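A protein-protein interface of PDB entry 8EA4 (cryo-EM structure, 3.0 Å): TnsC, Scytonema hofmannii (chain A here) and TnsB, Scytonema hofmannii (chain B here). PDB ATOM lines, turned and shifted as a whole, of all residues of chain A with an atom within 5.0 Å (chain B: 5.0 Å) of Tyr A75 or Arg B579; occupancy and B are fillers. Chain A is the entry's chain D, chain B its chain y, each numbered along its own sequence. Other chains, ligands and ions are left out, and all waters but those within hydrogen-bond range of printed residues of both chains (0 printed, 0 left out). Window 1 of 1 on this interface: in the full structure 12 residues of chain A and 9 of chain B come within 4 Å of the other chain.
The side-chain hydroxyl of Tyr B575 sits close to the side-chain carboxylate of Asp A71 (2.3 Å).
The side-chain carboxylate (OD1) of Asp A71 is in salt-bridge range of the guanidinium group (NH2) of Arg A74 (2.7 Å). The guanidinium group of Arg B579 is in salt-bridge range of the side-chain carboxylate of Glu B576, 2.8 Å away.
Arg A74 touches Tyr B582. Tyr A75 touches Leu B578 (CD2 to CB, 3.3 Å). CG of Arg B579 touches OH of Tyr A75 (3.0 Å). CD1 of Tyr A75 touches CD1 of Tyr B582 (3.0 Å).
Arg B579 touches one residue of chain A. Printed residues of chain A within 4 Å of Tyr B582: Arg A74 and Tyr A75. Of the printed residues of chain A, Tyr B575 touches Asp A71. Of the printed residues of chain B, Asp A71 touches Tyr B575 (2.3 Å). Of the printed residues of chain B, Arg A74 touches Tyr B582. Of the printed residues of chain A, Leu B578 touches Tyr A75. Ala A72 touches none of the printed residues of chain B. The nearest residue of chain B that does not touch Tyr A75 is Tyr B575 (4.4 Å). The nearest residue of chain A that does not touch Arg B579 is Asp A71 (4.2 Å).
Along chain A the printed residues that touch a printed residue of chain B span positions 71 to 75. Among the printed residues, 5 pairs touch across the chains. Among the printed residues, no Asp or Glu carboxylate lies within 4 Å of a Lys or Arg side-chain nitrogen of the other chain.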
ATOM      1  N   ASP A  71      -2.494  13.203  33.565  1.00  0.00           N
ATOM      2  CA  ASP A  71      -2.201  13.631  32.207  1.00  0.00           C
ATOM      3  C   ASP A  71      -2.390  15.129  32.032  1.00  0.00           C
ATOM      4  O   ASP A  71      -1.579  15.777  31.389  1.00  0.00           O
ATOM      5  CB  ASP A  71      -3.074  12.883  31.216  1.00  0.00           C
ATOM      6  CG  ASP A  71      -2.567  11.490  30.882  1.00  0.00           C
ATOM      7  OD1 ASP A  71      -1.394  11.185  31.183  1.00  0.00           O
ATOM      8  OD2 ASP A  71      -3.308  10.739  30.219  1.00  0.00           O
ATOM      9  N   ALA A  72      -3.394  15.733  32.651  1.00  0.00           N
ATOM     10  CA  ALA A  72      -3.530  17.176  32.671  1.00  0.00           C
ATOM     11  C   ALA A  72      -2.331  17.863  33.355  1.00  0.00           C
ATOM     12  O   ALA A  72      -2.066  19.028  33.087  1.00  0.00           O
ATOM     13  CB  ALA A  72      -4.850  17.514  33.336  1.00  0.00           C
ATOM     14  N   TYR A  73      -1.605  17.174  34.237  1.00  0.00           N
ATOM     15  CA  TYR A  73      -0.371  17.685  34.815  1.00  0.00           C
ATOM     16  C   TYR A  73       0.801  17.511  33.858  1.00  0.00           C
ATOM     17  O   TYR A  73       1.420  18.496  33.505  1.00  0.00           O
ATOM     18  CB  TYR A  73      -0.114  17.079  36.193  1.00  0.00           C
ATOM     19  CG  TYR A  73       0.887  17.869  37.002  1.00  0.00           C
ATOM     20  CD1 TYR A  73       0.600  19.192  37.353  1.00  0.00           C
ATOM     21  CD2 TYR A  73       2.109  17.297  37.377  1.00  0.00           C
ATOM     22  CE1 TYR A  73       1.529  19.948  38.078  1.00  0.00           C
ATOM     23  CE2 TYR A  73       3.044  18.052  38.098  1.00  0.00           C
ATOM     24  CZ  TYR A  73       2.745  19.374  38.462  1.00  0.00           C
ATOM     25  OH  TYR A  73       3.639  20.086  39.178  1.00  0.00           O
ATOM     26  N   ARG A  74       1.065  16.304  33.343  1.00  0.00           N
ATOM     27  CA  ARG A  74       2.115  16.030  32.337  1.00  0.00           C
ATOM     28  C   ARG A  74       1.998  16.910  31.080  1.00  0.00           C
ATOM     29  O   ARG A  74       3.028  17.239  30.513  1.00  0.00           O
ATOM     30  CB  ARG A  74       2.114  14.530  31.968  1.00  0.00           C
ATOM     31  CG  ARG A  74       2.915  14.262  30.684  1.00  0.00           C
ATOM     32  CD  ARG A  74       3.106  12.824  30.239  1.00  0.00           C
ATOM     33  NE  ARG A  74       1.837  12.090  30.107  1.00  0.00           N
ATOM     34  CZ  ARG A  74       1.531  11.213  29.181  1.00  0.00           C
ATOM     35  NH1 ARG A  74       2.302  10.964  28.169  1.00  0.00           N
ATOM     36  NH2 ARG A  74       0.437  10.534  29.263  1.00  0.00           N
ATOM     37  N   TYR A  75       0.797  17.212  30.583  1.00  0.00           N
ATOM     38  CA  TYR A  75       0.584  18.016  29.378  1.00  0.00           C
ATOM     39  C   TYR A  75       0.632  19.517  29.645  1.00  0.00           C
ATOM     40  O   TYR A  75       0.852  20.296  28.722  1.00  0.00           O
ATOM     41  CB  TYR A  75      -0.719  17.604  28.696  1.00  0.00           C
ATOM     42  CG  TYR A  75      -0.785  16.173  28.201  1.00  0.00           C
ATOM     43  CD1 TYR A  75       0.343  15.540  27.652  1.00  0.00           C
ATOM     44  CD2 TYR A  75      -2.013  15.496  28.226  1.00  0.00           C
ATOM     45  CE1 TYR A  75       0.252  14.240  27.132  1.00  0.00           C
ATOM     46  CE2 TYR A  75      -2.110  14.197  27.696  1.00  0.00           C
ATOM     47  CZ  TYR A  75      -0.980  13.568  27.148  1.00  0.00           C
ATOM     48  OH  TYR A  75      -1.088  12.324  26.625  1.00  0.00           O
ATOM     49  N   ARG A  76       0.475  19.974  30.891  1.00  0.00           N
ATOM     50  CA  ARG A  76       1.073  21.243  31.338  1.00  0.00           C
ATOM     51  C   ARG A  76       2.564  20.978  31.626  1.00  0.00           C
ATOM     52  O   ARG A  76       2.998  19.855  31.449  1.00  0.00           O
ATOM     53  CB  ARG A  76       0.240  21.762  32.513  1.00  0.00           C
ATOM     54  CG  ARG A  76       0.483  23.235  32.851  1.00  0.00           C
ATOM     55  CD  ARG A  76      -0.772  23.907  33.402  1.00  0.00           C
ATOM     56  NE  ARG A  76      -1.264  23.289  34.639  1.00  0.00           N
ATOM     57  CZ  ARG A  76      -1.250  23.810  35.840  1.00  0.00           C
ATOM     58  NH1 ARG A  76      -0.596  24.871  36.131  1.00  0.00           N
ATOM     59  NH2 ARG A  76      -1.929  23.282  36.790  1.00  0.00           N
ATOM     60  N   HIS A  77       3.400  21.943  32.006  1.00  0.00           N
ATOM     61  CA  HIS A  77       4.833  21.677  32.288  1.00  0.00           C
ATOM     62  C   HIS A  77       5.588  20.960  31.145  1.00  0.00           C
ATOM     63  O   HIS A  77       6.356  20.026  31.371  1.00  0.00           O
ATOM     64  CB  HIS A  77       5.011  20.969  33.646  1.00  0.00           C
ATOM     65  CG  HIS A  77       4.376  21.722  34.773  1.00  0.00           C
ATOM     66  ND1 HIS A  77       4.805  22.923  35.271  1.00  0.00           N
ATOM     67  CD2 HIS A  77       3.147  21.478  35.309  1.00  0.00           C
ATOM     68  CE1 HIS A  77       3.866  23.392  36.093  1.00  0.00           C
ATOM     69  NE2 HIS A  77       2.835  22.542  36.156  1.00  0.00           N
ATOM     70  N   LYS A  78       5.362  21.402  29.904  1.00  0.00           N
ATOM     71  CA  LYS A  78       5.933  20.822  28.675  1.00  0.00           C
ATOM     72  C   LYS A  78       7.472  20.745  28.724  1.00  0.00           C
ATOM     73  O   LYS A  78       8.087  21.696  29.205  1.00  0.00           O
ATOM     74  CB  LYS A  78       5.455  21.677  27.487  1.00  0.00           C
ATOM     75  CG  LYS A  78       5.693  20.996  26.132  1.00  0.00           C
ATOM     76  CD  LYS A  78       5.319  21.880  24.934  1.00  0.00           C
ATOM     77  CE  LYS A  78       6.249  23.082  24.707  1.00  0.00           C
ATOM     78  NZ  LYS A  78       7.609  22.703  24.234  1.00  0.00           N
ATOM     79  N   TYR B 575      -8.972  15.081  25.121  1.00  0.00           N
ATOM     80  CA  TYR B 575      -7.851  14.190  25.522  1.00  0.00           C
ATOM     81  C   TYR B 575      -6.836  14.098  24.375  1.00  0.00           C
ATOM     82  O   TYR B 575      -5.619  14.168  24.636  1.00  0.00           O
ATOM     83  CB  TYR B 575      -8.380  12.804  25.904  1.00  0.00           C
ATOM     84  CG  TYR B 575      -7.633  12.129  27.026  1.00  0.00           C
ATOM     85  CD1 TYR B 575      -6.610  12.779  27.699  1.00  0.00           C
ATOM     86  CD2 TYR B 575      -7.945  10.837  27.416  1.00  0.00           C
ATOM     87  CE1 TYR B 575      -5.919  12.165  28.730  1.00  0.00           C
ATOM     88  CE2 TYR B 575      -7.263  10.208  28.445  1.00  0.00           C
ATOM     89  CZ  TYR B 575      -6.246  10.875  29.104  1.00  0.00           C
ATOM     90  OH  TYR B 575      -5.570  10.261  30.120  1.00  0.00           O
ATOM     91  N   GLU B 576      -7.338  13.946  23.147  1.00  0.00           N
ATOM     92  CA  GLU B 576      -6.497  13.842  21.957  1.00  0.00           C
ATOM     93  C   GLU B 576      -5.825  15.169  21.571  1.00  0.00           C
ATOM     94  O   GLU B 576      -4.678  15.144  21.127  1.00  0.00           O
ATOM     95  CB  GLU B 576      -7.286  13.272  20.780  1.00  0.00           C
ATOM     96  CG  GLU B 576      -8.059  11.982  21.081  1.00  0.00           C
ATOM     97  CD  GLU B 576      -7.273  10.950  21.894  1.00  0.00           C
ATOM     98  OE1 GLU B 576      -6.057  10.789  21.688  1.00  0.00           O
ATOM     99  OE2 GLU B 576      -7.857  10.289  22.776  1.00  0.00           O
ATOM    100  N   GLN B 577      -6.459  16.334  21.776  1.00  0.00           N
ATOM    101  CA  GLN B 577      -5.720  17.576  21.616  1.00  0.00           C
ATOM    102  C   GLN B 577      -4.562  17.771  22.583  1.00  0.00           C
ATOM    103  O   GLN B 577      -3.445  18.069  22.169  1.00  0.00           O
ATOM    104  CB  GLN B 577      -6.688  18.755  21.747  1.00  0.00           C
ATOM    105  CG  GLN B 577      -6.032  20.117  21.582  1.00  0.00           C
ATOM    106  CD  GLN B 577      -7.018  21.258  21.758  1.00  0.00           C
ATOM    107  OE1 GLN B 577      -8.235  21.056  21.717  1.00  0.00           O
ATOM    108  NE2 GLN B 577      -6.495  22.462  21.953  1.00  0.00           N
ATOM    109  N   LEU B 578      -4.773  17.439  23.864  1.00  0.00           N
ATOM    110  CA  LEU B 578      -3.688  17.344  24.844  1.00  0.00           C
ATOM    111  C   LEU B 578      -2.551  16.431  24.373  1.00  0.00           C
ATOM    112  O   LEU B 578      -1.393  16.825  24.476  1.00  0.00           O
ATOM    113  CB  LEU B 578      -4.237  16.853  26.192  1.00  0.00           C
ATOM    114  CG  LEU B 578      -5.136  17.859  26.926  1.00  0.00           C
ATOM    115  CD1 LEU B 578      -5.769  17.174  28.125  1.00  0.00           C
ATOM    116  CD2 LEU B 578      -4.369  19.069  27.431  1.00  0.00           C
ATOM    117  N   ARG B 579      -2.847  15.260  23.797  1.00  0.00           N
ATOM    118  CA  ARG B 579      -1.827  14.403  23.170  1.00  0.00           C
ATOM    119  C   ARG B 579      -1.104  15.069  22.001  1.00  0.00           C
ATOM    120  O   ARG B 579       0.106  14.919  21.884  1.00  0.00           O
ATOM    121  CB  ARG B 579      -2.426  13.049  22.781  1.00  0.00           C
ATOM    122  CG  ARG B 579      -2.235  12.071  23.915  1.00  0.00           C
ATOM    123  CD  ARG B 579      -2.760  10.673  23.627  1.00  0.00           C
ATOM    124  NE  ARG B 579      -4.210  10.568  23.825  1.00  0.00           N
ATOM    125  CZ  ARG B 579      -4.852  10.414  24.960  1.00  0.00           C
ATOM    126  NH1 ARG B 579      -4.256  10.396  26.108  1.00  0.00           N
ATOM    127  NH2 ARG B 579      -6.132  10.270  24.961  1.00  0.00           N
ATOM    128  N   GLU B 580      -1.833  15.768  21.143  1.00  0.00           N
ATOM    129  CA  GLU B 580      -1.247  16.440  19.973  1.00  0.00           C
ATOM    130  C   GLU B 580      -0.319  17.619  20.326  1.00  0.00           C
ATOM    131  O   GLU B 580       0.722  17.825  19.719  1.00  0.00           O
ATOM    132  CB  GLU B 580      -2.374  16.894  19.021  1.00  0.00           C
ATOM    133  CG  GLU B 580      -1.836  17.557  17.750  1.00  0.00           C
ATOM    134  CD  GLU B 580      -2.989  17.916  16.769  1.00  0.00           C
ATOM    135  OE1 GLU B 580      -4.197  17.748  17.089  1.00  0.00           O
ATOM    136  OE2 GLU B 580      -2.712  18.377  15.635  1.00  0.00           O
ATOM    137  N   GLU B 581      -0.676  18.380  21.348  1.00  0.00           N
ATOM    138  CA  GLU B 581       0.083  19.483  21.938  1.00  0.00           C
ATOM    139  C   GLU B 581       1.281  19.027  22.788  1.00  0.00           C
ATOM    140  O   GLU B 581       2.119  19.852  23.147  1.00  0.00           O
ATOM    141  CB  GLU B 581      -0.870  20.325  22.798  1.00  0.00           C
ATOM    142  CG  GLU B 581      -1.885  21.091  21.942  1.00  0.00           C
ATOM    143  CD  GLU B 581      -2.846  21.978  22.748  1.00  0.00           C
ATOM    144  OE1 GLU B 581      -2.781  22.026  23.993  1.00  0.00           O
ATOM    145  OE2 GLU B 581      -3.682  22.665  22.123  1.00  0.00           O
ATOM    146  N   TYR B 582       1.366  17.759  23.195  1.00  0.00           N
ATOM    147  CA  TYR B 582       2.432  17.303  24.078  1.00  0.00           C
ATOM    148  C   TYR B 582       3.816  17.243  23.388  1.00  0.00           C
ATOM    149  O   TYR B 582       3.928  17.325  22.164  1.00  0.00           O
ATOM    150  CB  TYR B 582       2.020  15.982  24.739  1.00  0.00           C
ATOM    151  CG  TYR B 582       2.909  15.603  25.903  1.00  0.00           C
ATOM    152  CD1 TYR B 582       3.063  16.499  26.980  1.00  0.00           C
ATOM    153  CD2 TYR B 582       3.666  14.420  25.860  1.00  0.00           C
ATOM    154  CE1 TYR B 582       3.982  16.211  27.998  1.00  0.00           C
ATOM    155  CE2 TYR B 582       4.592  14.140  26.873  1.00  0.00           C
ATOM    156  CZ  TYR B 582       4.760  15.046  27.938  1.00  0.00           C
ATOM    157  OH  TYR B 582       5.671  14.800  28.902  1.00  0.00           O
